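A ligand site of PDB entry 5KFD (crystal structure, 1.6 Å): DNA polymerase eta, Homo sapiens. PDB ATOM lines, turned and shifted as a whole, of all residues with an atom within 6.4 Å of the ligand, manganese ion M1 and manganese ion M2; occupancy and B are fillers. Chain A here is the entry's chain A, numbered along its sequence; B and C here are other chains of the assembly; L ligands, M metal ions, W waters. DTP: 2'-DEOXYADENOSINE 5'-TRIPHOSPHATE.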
ATOM      1  N   ASP A  16       2.127 -34.323 -12.211  1.00  0.00           N
ATOM      2  CA  ASP A  16       2.496 -33.444 -11.109  1.00  0.00           C
ATOM      3  C   ASP A  16       2.304 -31.979 -11.479  1.00  0.00           C
ATOM      4  O   ASP A  16       2.848 -31.488 -12.464  1.00  0.00           O
ATOM      5  CB  ASP A  16       3.942 -33.685 -10.686  1.00  0.00           C
ATOM      6  CG  ASP A  16       4.366 -32.795  -9.559  1.00  0.00           C
ATOM      7  OD1 ASP A  16       4.822 -31.676  -9.844  1.00  0.00           O
ATOM      8  OD2 ASP A  16       4.222 -33.203  -8.385  1.00  0.00           O
ATOM      9  N   MET A  17       1.530 -31.243 -10.678  1.00  0.00           N
ATOM     10  CA  MET A  17       1.230 -29.848 -11.037  1.00  0.00           C
ATOM     11  C   MET A  17       2.478 -28.975 -10.971  1.00  0.00           C
ATOM     12  O   MET A  17       3.333 -29.163 -10.115  1.00  0.00           O
ATOM     13  CB  MET A  17       0.154 -29.271 -10.112  1.00  0.00           C
ATOM     14  CG  MET A  17      -1.078 -30.121 -10.009  1.00  0.00           C
ATOM     15  SD  MET A  17      -1.841 -30.521 -11.595  1.00  0.00           S
ATOM     16  CE  MET A  17      -2.328 -28.936 -12.177  1.00  0.00           C
ATOM     17  N   ASP A  18       2.601 -28.022 -11.895  1.00  0.00           N
ATOM     18  CA  ASP A  18       3.741 -27.098 -11.848  1.00  0.00           C
ATOM     19  C   ASP A  18       3.543 -26.026 -10.788  1.00  0.00           C
ATOM     20  O   ASP A  18       2.494 -25.385 -10.772  1.00  0.00           O
ATOM     21  CB  ASP A  18       3.937 -26.395 -13.180  1.00  0.00           C
ATOM     22  CG  ASP A  18       4.241 -27.369 -14.323  1.00  0.00           C
ATOM     23  OD1 ASP A  18       4.846 -28.424 -14.078  1.00  0.00           O
ATOM     24  OD2 ASP A  18       3.891 -27.047 -15.474  1.00  0.00           O
ATOM     25  N   CYS A  19       4.554 -25.848  -9.930  1.00  0.00           N
ATOM     26  CA  CYS A  19       4.553 -24.865  -8.829  1.00  0.00           C
ATOM     27  C   CYS A  19       3.134 -24.632  -8.280  1.00  0.00           C
ATOM     28  O   CYS A  19       2.590 -23.534  -8.369  1.00  0.00           O
ATOM     29  CB  CYS A  19       5.211 -23.523  -9.228  1.00  0.00           C
ATOM     30  SG  CYS A  19       4.627 -22.708 -10.740  1.00  0.00           S
ATOM     31  N   PHE A  20       2.559 -25.691  -7.721  1.00  0.00           N
ATOM     32  CA  PHE A  20       1.106 -25.802  -7.578  1.00  0.00           C
ATOM     33  C   PHE A  20       0.438 -24.662  -6.780  1.00  0.00           C
ATOM     34  O   PHE A  20      -0.460 -23.995  -7.323  1.00  0.00           O
ATOM     35  CB  PHE A  20       0.731 -27.152  -6.957  1.00  0.00           C
ATOM     36  CG  PHE A  20      -0.761 -27.371  -6.840  1.00  0.00           C
ATOM     37  CD1 PHE A  20      -1.599 -27.099  -7.910  1.00  0.00           C
ATOM     38  CD2 PHE A  20      -1.314 -27.833  -5.653  1.00  0.00           C
ATOM     39  CE1 PHE A  20      -2.985 -27.296  -7.793  1.00  0.00           C
ATOM     40  CE2 PHE A  20      -2.692 -28.024  -5.538  1.00  0.00           C
ATOM     41  CZ  PHE A  20      -3.519 -27.769  -6.609  1.00  0.00           C
ATOM     42  N   PHE A  21       0.881 -24.401  -5.551  1.00  0.00           N
ATOM     43  CA  PHE A  21       0.235 -23.367  -4.745  1.00  0.00           C
ATOM     44  C   PHE A  21       0.355 -22.001  -5.409  1.00  0.00           C
ATOM     45  O   PHE A  21      -0.537 -21.180  -5.290  1.00  0.00           O
ATOM     46  CB  PHE A  21       0.821 -23.289  -3.309  1.00  0.00           C
ATOM     47  CG  PHE A  21       0.484 -24.452  -2.422  1.00  0.00           C
ATOM     48  CD1 PHE A  21      -0.053 -25.634  -2.922  1.00  0.00           C
ATOM     49  CD2 PHE A  21       0.711 -24.353  -1.059  1.00  0.00           C
ATOM     50  CE1 PHE A  21      -0.351 -26.697  -2.060  1.00  0.00           C
ATOM     51  CE2 PHE A  21       0.407 -25.408  -0.196  1.00  0.00           C
ATOM     52  CZ  PHE A  21      -0.112 -26.579  -0.698  1.00  0.00           C
ATOM     53  N   VAL A  22       1.470 -21.764  -6.110  1.00  0.00           N
ATOM     54  CA  VAL A  22       1.651 -20.522  -6.850  1.00  0.00           C
ATOM     55  C   VAL A  22       0.601 -20.410  -7.957  1.00  0.00           C
ATOM     56  O   VAL A  22      -0.021 -19.356  -8.150  1.00  0.00           O
ATOM     57  CB  VAL A  22       3.065 -20.408  -7.442  1.00  0.00           C
ATOM     58  CG1 VAL A  22       3.117 -19.345  -8.569  1.00  0.00           C
ATOM     59  CG2 VAL A  22       4.085 -20.096  -6.344  1.00  0.00           C
ATOM     60  N   GLN A  41       4.039 -18.741   4.151  1.00  0.00           N
ATOM     61  CA  GLN A  41       3.171 -18.856   5.318  1.00  0.00           C
ATOM     62  C   GLN A  41       3.757 -18.078   6.479  1.00  0.00           C
ATOM     63  O   GLN A  41       4.965 -18.080   6.714  1.00  0.00           O
ATOM     64  CB  GLN A  41       2.880 -20.317   5.709  1.00  0.00           C
ATOM     65  CG  GLN A  41       4.048 -21.246   5.813  1.00  0.00           C
ATOM     66  CD  GLN A  41       3.607 -22.699   5.858  1.00  0.00           C
ATOM     67  OE1 GLN A  41       2.436 -23.044   5.610  1.00  0.00           O
ATOM     68  NE2 GLN A  41       4.531 -23.565   6.208  1.00  0.00           N
ATOM     69  N   ILE A  51       6.900 -21.637   0.639  1.00  0.00           N
ATOM     70  CA  ILE A  51       6.573 -23.034   0.410  1.00  0.00           C
ATOM     71  C   ILE A  51       6.321 -23.370  -1.070  1.00  0.00           C
ATOM     72  O   ILE A  51       6.208 -24.547  -1.413  1.00  0.00           O
ATOM     73  CB  ILE A  51       5.358 -23.500   1.244  1.00  0.00           C
ATOM     74  CG1 ILE A  51       4.095 -22.680   0.940  1.00  0.00           C
ATOM     75  CG2 ILE A  51       5.683 -23.453   2.748  1.00  0.00           C
ATOM     76  CD1 ILE A  51       2.849 -23.296   1.566  1.00  0.00           C
ATOM     77  N   ALA A  52       6.250 -22.368  -1.933  1.00  0.00           N
ATOM     78  CA  ALA A  52       6.136 -22.615  -3.377  1.00  0.00           C
ATOM     79  C   ALA A  52       6.662 -21.430  -4.173  1.00  0.00           C
ATOM     80  O   ALA A  52       6.529 -20.286  -3.744  1.00  0.00           O
ATOM     81  CB  ALA A  52       4.672 -22.926  -3.785  1.00  0.00           C
ATOM     82  N   VAL A  53       7.290 -21.712  -5.323  1.00  0.00           N
ATOM     83  CA  VAL A  53       8.037 -20.708  -6.071  1.00  0.00           C
ATOM     84  C   VAL A  53       7.765 -20.816  -7.570  1.00  0.00           C
ATOM     85  O   VAL A  53       7.930 -21.905  -8.145  1.00  0.00           O
ATOM     86  CB  VAL A  53       9.563 -20.884  -5.848  1.00  0.00           C
ATOM     87  CG1 VAL A  53      10.343 -19.746  -6.469  1.00  0.00           C
ATOM     88  CG2 VAL A  53       9.887 -21.017  -4.343  1.00  0.00           C
ATOM     89  N   TYR A  55       8.426 -20.403 -11.604  1.00  0.00           N
ATOM     90  CA  TYR A  55       9.650 -20.667 -12.364  1.00  0.00           C
ATOM     91  C   TYR A  55      10.404 -19.386 -12.692  1.00  0.00           C
ATOM     92  O   TYR A  55      11.628 -19.384 -12.720  1.00  0.00           O
ATOM     93  CB  TYR A  55       9.343 -21.483 -13.624  1.00  0.00           C
ATOM     94  CG  TYR A  55       9.146 -22.928 -13.274  1.00  0.00           C
ATOM     95  CD1 TYR A  55       7.940 -23.367 -12.753  1.00  0.00           C
ATOM     96  CD2 TYR A  55      10.206 -23.832 -13.350  1.00  0.00           C
ATOM     97  CE1 TYR A  55       7.767 -24.679 -12.365  1.00  0.00           C
ATOM     98  CE2 TYR A  55      10.037 -25.152 -12.972  1.00  0.00           C
ATOM     99  CZ  TYR A  55       8.823 -25.584 -12.481  1.00  0.00           C
ATOM    100  OH  TYR A  55       8.657 -26.890 -12.104  1.00  0.00           O
ATOM    101  N   ARG A  58      12.396 -18.827  -9.576  1.00  0.00           N
ATOM    102  CA  ARG A  58      13.474 -19.808  -9.402  1.00  0.00           C
ATOM    103  C   ARG A  58      14.734 -19.378 -10.150  1.00  0.00           C
ATOM    104  O   ARG A  58      15.862 -19.706  -9.743  1.00  0.00           O
ATOM    105  CB  ARG A  58      13.051 -21.193  -9.872  1.00  0.00           C
ATOM    106  CG  ARG A  58      11.888 -21.729  -9.104  1.00  0.00           C
ATOM    107  CD  ARG A  58      11.495 -23.119  -9.557  1.00  0.00           C
ATOM    108  NE  ARG A  58      10.179 -23.442  -9.005  1.00  0.00           N
ATOM    109  CZ  ARG A  58       9.631 -24.651  -9.001  1.00  0.00           C
ATOM    110  NH1 ARG A  58      10.302 -25.675  -9.518  1.00  0.00           N
ATOM    111  NH2 ARG A  58       8.423 -24.830  -8.461  1.00  0.00           N
ATOM    112  N   ARG A  64      12.046 -23.073  -2.094  1.00  0.00           N
ATOM    113  CA  ARG A  64      11.314 -23.519  -0.919  1.00  0.00           C
ATOM    114  C   ARG A  64      12.208 -23.502   0.325  1.00  0.00           C
ATOM    115  O   ARG A  64      13.428 -23.689   0.218  1.00  0.00           O
ATOM    116  CB  ARG A  64      10.762 -24.930  -1.185  1.00  0.00           C
ATOM    117  CG  ARG A  64      10.088 -25.612  -0.014  1.00  0.00           C
ATOM    118  CD  ARG A  64       9.432 -26.913  -0.461  1.00  0.00           C
ATOM    119  NE  ARG A  64       8.326 -26.588  -1.342  1.00  0.00           N
ATOM    120  CZ  ARG A  64       8.087 -27.149  -2.531  1.00  0.00           C
ATOM    121  NH1 ARG A  64       8.875 -28.110  -3.020  1.00  0.00           N
ATOM    122  NH2 ARG A  64       7.044 -26.746  -3.238  1.00  0.00           N
ATOM    123  N   LEU A  92      -4.758 -24.743   4.866  1.00  0.00           N
ATOM    124  CA  LEU A  92      -4.455 -25.102   3.469  1.00  0.00           C
ATOM    125  C   LEU A  92      -5.681 -25.481   2.624  1.00  0.00           C
ATOM    126  O   LEU A  92      -5.539 -26.088   1.567  1.00  0.00           O
ATOM    127  CB  LEU A  92      -3.455 -26.253   3.441  1.00  0.00           C
ATOM    128  CG  LEU A  92      -2.183 -26.022   4.252  1.00  0.00           C
ATOM    129  CD1 LEU A  92      -1.302 -27.263   4.247  1.00  0.00           C
ATOM    130  CD2 LEU A  92      -1.446 -24.809   3.695  1.00  0.00           C
ATOM    131  N   SER A 116       0.142 -37.132  -3.490  1.00  0.00           N
ATOM    132  CA  SER A 116       0.365 -35.922  -2.706  1.00  0.00           C
ATOM    133  C   SER A 116      -0.744 -34.939  -3.038  1.00  0.00           C
ATOM    134  O   SER A 116      -1.631 -35.220  -3.828  1.00  0.00           O
ATOM    135  CB  SER A 116       1.722 -35.276  -3.013  1.00  0.00           C
ATOM    136  OG  SER A 116       1.670 -34.562  -4.249  1.00  0.00           O
ATOM    137  N   ILE A 117      -0.677 -33.760  -2.438  1.00  0.00           N
ATOM    138  CA  ILE A 117      -1.680 -32.747  -2.731  1.00  0.00           C
ATOM    139  C   ILE A 117      -1.637 -32.326  -4.206  1.00  0.00           C
ATOM    140  O   ILE A 117      -2.631 -31.842  -4.748  1.00  0.00           O
ATOM    141  CB  ILE A 117      -1.487 -31.491  -1.833  1.00  0.00           C
ATOM    142  CG1 ILE A 117      -2.773 -30.672  -1.804  1.00  0.00           C
ATOM    143  CG2 ILE A 117      -0.280 -30.660  -2.286  1.00  0.00           C
ATOM    144  CD1 ILE A 117      -2.798 -29.583  -0.721  1.00  0.00           C
ATOM    145  N   ASP A 118      -0.514 -32.517  -4.896  1.00  0.00           N
ATOM    146  CA  ASP A 118      -0.500 -32.037  -6.278  1.00  0.00           C
ATOM    147  C   ASP A 118      -0.077 -33.083  -7.312  1.00  0.00           C
ATOM    148  O   ASP A 118       0.269 -32.737  -8.446  1.00  0.00           O
ATOM    149  CB  ASP A 118       0.389 -30.800  -6.398  1.00  0.00           C
ATOM    150  CG  ASP A 118       1.847 -31.133  -6.660  1.00  0.00           C
ATOM    151  OD1 ASP A 118       2.373 -32.151  -6.126  1.00  0.00           O
ATOM    152  OD2 ASP A 118       2.447 -30.412  -7.491  1.00  0.00           O
ATOM    153  N   GLU A 119      -0.125 -34.370  -6.957  1.00  0.00           N
ATOM    154  CA  GLU A 119       0.240 -35.374  -7.945  1.00  0.00           C
ATOM    155  C   GLU A 119      -0.449 -36.701  -7.735  1.00  0.00           C
ATOM    156  O   GLU A 119      -0.860 -37.041  -6.614  1.00  0.00           O
ATOM    157  CB  GLU A 119       1.740 -35.587  -7.960  1.00  0.00           C
ATOM    158  CG  GLU A 119       2.260 -36.420  -6.814  1.00  0.00           C
ATOM    159  CD  GLU A 119       3.700 -36.071  -6.504  1.00  0.00           C
ATOM    160  OE1 GLU A 119       4.614 -36.838  -6.867  1.00  0.00           O
ATOM    161  OE2 GLU A 119       3.912 -35.000  -5.899  1.00  0.00           O
ATOM    162  N   SER A 216       3.223 -31.167 -15.361  1.00  0.00           N
ATOM    163  CA  SER A 216       4.159 -32.006 -16.077  1.00  0.00           C
ATOM    164  C   SER A 216       3.784 -33.453 -15.819  1.00  0.00           C
ATOM    165  O   SER A 216       2.998 -33.737 -14.920  1.00  0.00           O
ATOM    166  CB  SER A 216       5.583 -31.722 -15.645  1.00  0.00           C
ATOM    167  OG  SER A 216       5.889 -30.355 -15.916  1.00  0.00           O
ATOM    168  N   LYS A 227       7.682 -41.243 -12.021  1.00  0.00           N
ATOM    169  CA  LYS A 227       8.028 -40.099 -11.178  1.00  0.00           C
ATOM    170  C   LYS A 227       9.351 -39.457 -11.602  1.00  0.00           C
ATOM    171  O   LYS A 227       9.431 -38.235 -11.728  1.00  0.00           O
ATOM    172  CB  LYS A 227       8.104 -40.537  -9.706  1.00  0.00           C
ATOM    173  CG  LYS A 227       8.517 -39.405  -8.760  1.00  0.00           C
ATOM    174  CD  LYS A 227       7.506 -38.259  -8.751  1.00  0.00           C
ATOM    175  CE  LYS A 227       8.031 -37.095  -7.908  1.00  0.00           C
ATOM    176  NZ  LYS A 227       7.060 -35.982  -7.732  1.00  0.00           N
ATOM    177  N   LYS A 234      10.376 -30.333 -16.719  1.00  0.00           N
ATOM    178  CA  LYS A 234       9.456 -29.329 -16.186  1.00  0.00           C
ATOM    179  C   LYS A 234       9.818 -27.883 -16.564  1.00  0.00           C
ATOM    180  O   LYS A 234      10.964 -27.574 -16.766  1.00  0.00           O
ATOM    181  CB  LYS A 234       9.448 -29.395 -14.656  1.00  0.00           C
ATOM    182  CG  LYS A 234       8.955 -30.656 -14.024  1.00  0.00           C
ATOM    183  CD  LYS A 234       8.874 -30.496 -12.468  1.00  0.00           C
ATOM    184  CE  LYS A 234      10.180 -29.889 -11.935  1.00  0.00           C
ATOM    185  NZ  LYS A 234      10.460 -29.848 -10.436  1.00  0.00           N
ATOM    186  N   PRO A 235       8.869 -26.982 -16.590  1.00  0.00           N
ATOM    187  CA  PRO A 235       7.434 -27.146 -16.388  1.00  0.00           C
ATOM    188  C   PRO A 235       6.693 -27.369 -17.697  1.00  0.00           C
ATOM    189  O   PRO A 235       7.260 -27.204 -18.783  1.00  0.00           O
ATOM    190  CB  PRO A 235       7.026 -25.811 -15.780  1.00  0.00           C
ATOM    191  CG  PRO A 235       7.922 -24.830 -16.513  1.00  0.00           C
ATOM    192  CD  PRO A 235       9.243 -25.568 -16.718  1.00  0.00           C
ATOM    193  P    DT B   8       9.283 -35.731  -3.040  1.00  0.00           P
ATOM    194  OP1  DT B   8       9.387 -35.785  -4.518  1.00  0.00           O
ATOM    195  OP2  DT B   8      10.272 -34.952  -2.263  1.00  0.00           O
ATOM    196  O5'  DT B   8       7.828 -35.155  -2.609  1.00  0.00           O
ATOM    197  C5'  DT B   8       6.548 -35.637  -3.145  1.00  0.00           C
ATOM    198  C4'  DT B   8       5.485 -34.623  -2.748  1.00  0.00           C
ATOM    199  O4'  DT B   8       5.633 -34.484  -1.316  1.00  0.00           O
ATOM    200  C3'  DT B   8       5.837 -33.275  -3.376  1.00  0.00           C
ATOM    201  O3'  DT B   8       4.697 -32.735  -4.044  1.00  0.00           O
ATOM    202  C2'  DT B   8       6.261 -32.390  -2.178  1.00  0.00           C
ATOM    203  C1'  DT B   8       5.640 -33.112  -0.983  1.00  0.00           C
ATOM    204  N1   DT B   8       6.421 -32.919   0.281  1.00  0.00           N
ATOM    205  C2   DT B   8       5.804 -32.302   1.358  1.00  0.00           C
ATOM    206  O2   DT B   8       4.651 -31.894   1.326  1.00  0.00           O
ATOM    207  N3   DT B   8       6.593 -32.166   2.471  1.00  0.00           N
ATOM    208  C4   DT B   8       7.903 -32.574   2.617  1.00  0.00           C
ATOM    209  O4   DT B   8       8.524 -32.413   3.658  1.00  0.00           O
ATOM    210  C5   DT B   8       8.486 -33.208   1.454  1.00  0.00           C
ATOM    211  C7   DT B   8       9.904 -33.706   1.499  1.00  0.00           C
ATOM    212  C6   DT B   8       7.718 -33.356   0.359  1.00  0.00           C
ATOM    213  P    DT C   3      15.331 -22.684  10.882  1.00  0.00           P
ATOM    214  OP1  DT C   3      15.873 -23.716  11.806  1.00  0.00           O
ATOM    215  OP2  DT C   3      16.228 -21.731  10.209  1.00  0.00           O
ATOM    216  O5'  DT C   3      14.450 -23.444   9.782  1.00  0.00           O
ATOM    217  C5'  DT C   3      13.511 -22.717   9.012  1.00  0.00           C
ATOM    218  C4'  DT C   3      12.580 -23.665   8.290  1.00  0.00           C
ATOM    219  O4'  DT C   3      13.255 -24.253   7.157  1.00  0.00           O
ATOM    220  C3'  DT C   3      12.090 -24.842   9.143  1.00  0.00           C
ATOM    221  O3'  DT C   3      10.664 -24.814   9.262  1.00  0.00           O
ATOM    222  C2'  DT C   3      12.584 -26.089   8.414  1.00  0.00           C
ATOM    223  C1'  DT C   3      12.841 -25.580   7.007  1.00  0.00           C
ATOM    224  N1   DT C   3      13.901 -26.314   6.307  1.00  0.00           N
ATOM    225  C2   DT C   3      13.602 -26.963   5.135  1.00  0.00           C
ATOM    226  O2   DT C   3      12.488 -26.980   4.649  1.00  0.00           O
ATOM    227  N3   DT C   3      14.661 -27.621   4.555  1.00  0.00           N
ATOM    228  C4   DT C   3      15.962 -27.672   5.022  1.00  0.00           C
ATOM    229  O4   DT C   3      16.850 -28.274   4.430  1.00  0.00           O
ATOM    230  C5   DT C   3      16.214 -26.961   6.249  1.00  0.00           C
ATOM    231  C7   DT C   3      17.586 -26.951   6.859  1.00  0.00           C
ATOM    232  C6   DT C   3      15.180 -26.323   6.826  1.00  0.00           C
ATOM    233  P    DT C   4      10.017 -24.635  10.716  1.00  0.00           P
ATOM    234  OP1  DT C   4      10.501 -23.348  11.272  1.00  0.00           O
ATOM    235  OP2  DT C   4      10.259 -25.900  11.442  1.00  0.00           O
ATOM    236  O5'  DT C   4       8.428 -24.571  10.450  1.00  0.00           O
ATOM    237  C5'  DT C   4       7.767 -23.324  10.191  1.00  0.00           C
ATOM    238  C4'  DT C   4       6.379 -23.597   9.604  1.00  0.00           C
ATOM    239  O4'  DT C   4       6.541 -24.286   8.344  1.00  0.00           O
ATOM    240  C3'  DT C   4       5.501 -24.514  10.455  1.00  0.00           C
ATOM    241  O3'  DT C   4       4.154 -24.150  10.253  1.00  0.00           O
ATOM    242  C2'  DT C   4       5.813 -25.900   9.867  1.00  0.00           C
ATOM    243  C1'  DT C   4       5.928 -25.552   8.395  1.00  0.00           C
ATOM    244  N1   DT C   4       6.743 -26.463   7.571  1.00  0.00           N
ATOM    245  C2   DT C   4       6.353 -26.649   6.286  1.00  0.00           C
ATOM    246  O2   DT C   4       5.340 -26.159   5.826  1.00  0.00           O
ATOM    247  N3   DT C   4       7.170 -27.443   5.531  1.00  0.00           N
ATOM    248  C4   DT C   4       8.335 -28.046   5.925  1.00  0.00           C
ATOM    249  O4   DT C   4       9.004 -28.745   5.165  1.00  0.00           O
ATOM    250  C5   DT C   4       8.734 -27.787   7.299  1.00  0.00           C
ATOM    251  C7   DT C   4       9.991 -28.411   7.855  1.00  0.00           C
ATOM    252  C6   DT C   4       7.928 -27.010   8.053  1.00  0.00           C
ATOM    253  P    DA C   5       2.974 -24.913  11.034  1.00  0.00           P
ATOM    254  OP1  DA C   5       1.995 -23.880  11.433  1.00  0.00           O
ATOM    255  OP2  DA C   5       3.552 -25.820  12.045  1.00  0.00           O
ATOM    256  O5'  DA C   5       2.339 -25.832   9.900  1.00  0.00           O
ATOM    257  C5'  DA C   5       1.669 -25.220   8.790  1.00  0.00           C
ATOM    258  C4'  DA C   5       1.043 -26.293   7.907  1.00  0.00           C
ATOM    259  O4'  DA C   5       2.087 -27.024   7.188  1.00  0.00           O
ATOM    260  C3'  DA C   5       0.249 -27.352   8.670  1.00  0.00           C
ATOM    261  O3'  DA C   5      -0.846 -27.756   7.872  1.00  0.00           O
ATOM    262  C2'  DA C   5       1.270 -28.488   8.810  1.00  0.00           C
ATOM    263  C1'  DA C   5       1.953 -28.397   7.451  1.00  0.00           C
ATOM    264  N9   DA C   5       3.276 -29.001   7.416  1.00  0.00           N
ATOM    265  C8   DA C   5       4.198 -29.046   8.416  1.00  0.00           C
ATOM    266  N7   DA C   5       5.322 -29.653   8.080  1.00  0.00           N
ATOM    267  C5   DA C   5       5.109 -30.021   6.757  1.00  0.00           C
ATOM    268  C6   DA C   5       5.910 -30.694   5.822  1.00  0.00           C
ATOM    269  N6   DA C   5       7.146 -31.134   6.087  1.00  0.00           N
ATOM    270  N1   DA C   5       5.384 -30.901   4.592  1.00  0.00           N
ATOM    271  C2   DA C   5       4.157 -30.456   4.326  1.00  0.00           C
ATOM    272  N3   DA C   5       3.308 -29.806   5.125  1.00  0.00           N
ATOM    273  C4   DA C   5       3.856 -29.618   6.333  1.00  0.00           C
HETATM  274  PG  DTP L   1       7.240 -28.115  -9.113  1.00  0.00           P
HETATM  275  O1G DTP L   1       6.573 -29.438  -8.915  1.00  0.00           O
HETATM  276  O2G DTP L   1       6.864 -27.452 -10.424  1.00  0.00           O
HETATM  277  O3G DTP L   1       8.753 -28.255  -9.009  1.00  0.00           O
HETATM  278  PB  DTP L   1       5.763 -27.482  -6.769  1.00  0.00           P
HETATM  279  O1B DTP L   1       4.452 -27.981  -7.363  1.00  0.00           O
HETATM  280  O2B DTP L   1       5.518 -26.220  -5.987  1.00  0.00           O
HETATM  281  O3B DTP L   1       6.821 -27.123  -7.928  1.00  0.00           O
HETATM  282  PA  DTP L   1       5.933 -29.909  -5.255  1.00  0.00           P
HETATM  283  O1A DTP L   1       5.305 -30.755  -6.331  1.00  0.00           O
HETATM  284  O2A DTP L   1       7.124 -30.582  -4.602  1.00  0.00           O
HETATM  285  O3A DTP L   1       6.500 -28.531  -5.825  1.00  0.00           O
HETATM  286  O5' DTP L   1       4.868 -29.575  -4.150  1.00  0.00           O
HETATM  287  C5' DTP L   1       3.534 -29.268  -4.474  1.00  0.00           C
HETATM  288  C4' DTP L   1       2.958 -28.271  -3.474  1.00  0.00           C
HETATM  289  O4' DTP L   1       2.996 -28.843  -2.178  1.00  0.00           O
HETATM  290  C3' DTP L   1       3.723 -27.032  -3.411  1.00  0.00           C
HETATM  291  O3' DTP L   1       3.244 -26.042  -4.331  1.00  0.00           O
HETATM  292  C2' DTP L   1       3.595 -26.557  -2.022  1.00  0.00           C
HETATM  293  C1' DTP L   1       3.419 -27.821  -1.263  1.00  0.00           C
HETATM  294  N9  DTP L   1       4.631 -28.240  -0.634  1.00  0.00           N
HETATM  295  C8  DTP L   1       5.629 -28.964  -1.187  1.00  0.00           C
HETATM  296  N7  DTP L   1       6.599 -29.174  -0.302  1.00  0.00           N
HETATM  297  C5  DTP L   1       6.248 -28.616   0.868  1.00  0.00           C
HETATM  298  C6  DTP L   1       6.821 -28.511   2.125  1.00  0.00           C
HETATM  299  N6  DTP L   1       8.103 -29.099   2.366  1.00  0.00           N
HETATM  300  N1  DTP L   1       6.184 -27.864   3.093  1.00  0.00           N
HETATM  301  C2  DTP L   1       4.977 -27.290   2.904  1.00  0.00           C
HETATM  302  N3  DTP L   1       4.377 -27.367   1.681  1.00  0.00           N
HETATM  303  C4  DTP L   1       4.990 -28.003   0.675  1.00  0.00           C
HETATM  304 MN    MN M   1       4.461 -32.937  -6.330  1.00  0.00          MN
HETATM  305 MN    MN M   2       4.423 -30.040  -8.424  1.00  0.00          MN
HETATM  306  O   HOH W   1       9.263 -30.270  -0.424  1.00  0.00           O
HETATM  307  O   HOH W   2       6.585 -33.376  -6.531  1.00  0.00           O
HETATM  308  O   HOH W   3       7.527 -24.473  -5.785  1.00  0.00           O
HETATM  309  O   HOH W   4       1.654 -26.930   2.336  1.00  0.00           O
HETATM  310  O   HOH W   5       7.944 -31.747  -8.372  1.00  0.00           O
HETATM  311  O   HOH W   6      10.232 -28.026  -6.753  1.00  0.00           O
HETATM  312  O   HOH W   7       2.979 -31.767  -2.310  1.00  0.00           O
HETATM  313  O   HOH W   8       2.503 -30.534   0.709  1.00  0.00           O
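Ser 116 touches manganese ion M1 (OG to MN, 3.8 Å).
The nearest printed residue that does not touch manganese ion M1 is Lys 227 (4.2 Å).
Three residues have an atom within 4 Å of manganese ion M2: Asp 16, Met 17 and Asp 118.
The nearest printed residue that does not touch manganese ion M2 is Asp 18 (4.4 Å).
OD2 of Asp 16 binds manganese ion M1.
Water W2 is bound to manganese ion M1 (2.2 Å).
Manganese ion M1 is bound by OE2 of Glu 119.
Manganese ion M1 is bound by the side-chain carboxylate (OD1) of Asp 118 (2.2 Å).
O3' of DT 8 of chain B binds manganese ion M1 (2.3 Å).
An oxygen (O1A) of the ligand binds manganese ion M1, at 2.3 Å.
Manganese ion M1 has six donor atoms within binding distance.
N of Phe 21 lies within hydrogen-bond range of O3' of the ligand, at 3.1 Å.
An oxygen (O2G) of the ligand lies within hydrogen-bond range of the backbone NH (N) of Cys 19 (2.9 Å).
An oxygen (O2B) of the ligand sits at hydrogen-bond distance from the backbone NH (N) of Phe 20 (3.5 Å).
The side-chain hydroxyl (OH) of Tyr 55 is in hydrogen-bond range of an oxygen (O2G) of the ligand (2.5 Å).
N3 of DT 8 of chain B lies within hydrogen-bond range of N6 of the ligand.
An oxygen (O2B) of the ligand is in salt-bridge range of the guanidinium group of Arg 64 (3.2 Å).
NZ of Lys 234 is in salt-bridge range of O3G of the ligand (2.7 Å).
O4 of DT 4 of chain C sits at hydrogen-bond distance from a nitrogen (N6) of the ligand (3.0 Å).
The guanidinium group (NH1) of Arg 58 is in salt-bridge range of an oxygen (O3G) of the ligand (3.1 Å).
Manganese ion M2 is bound by O of Met 17 (2.2 Å), OD1 of Asp 16 (2.2 Å), OD2 of Asp 118 (2.2 Å), O1G of the ligand (2.3 Å), O1B of the ligand (2.3 Å) and O1A of the ligand (2.4 Å).
N1 of DA 5 of chain C lies close to a nitrogen (N1) of the ligand.
Residues that only touch the ligand: Ile 51, Asp 18, Ala 52 and Ile 117.
Hydrophobic or aromatic side chains that line the ligand: Phe 20, Phe 21, Ile 51, Ala 52, Tyr 55 and Ile 117.
Of the 27 residues printed, 17 come within 4 Å of the ligand.
O of Ser 216 sits at hydrogen-bond distance from N of Asp 16, at 2.9 Å.
NH1 of Arg 58 is in hydrogen-bond range of OH of Tyr 55, at 3.3 Å.
The side-chain hydroxyl of Ser 116 lies close to the backbone NH of Glu 119 (3.3 Å).
The side-chain amide nitrogen of Gln 41 is in hydrogen-bond range of O2 of DT 4 of chain C (2.7 Å).
The side-chain hydroxyl of Ser 116 lies close to the backbone NH of Asp 118, at 3.1 Å.
OP1 of DT 8 of chain B lies within salt-bridge range of the side-chain amino group of Lys 227 (3.97 Å).
The guanidinium group (NE) of Arg 58 is in hydrogen-bond range of the backbone carbonyl oxygen (O) of Val 53 (2.9 Å).
NE of Arg 64 lies within hydrogen-bond range of O of Ile 51 (2.9 Å).
Water W2 bridges NZ of Lys 227 (2.9 Å) and O2A of the ligand (3.4 Å).
Water W1 bridges a nitrogen (N7) of the ligand (2.9 Å) and the guanidinium group of Arg 64 (3.4 Å).
Water W8 bridges O2 of DT 8 of chain B and an oxygen (O4') of the ligand.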
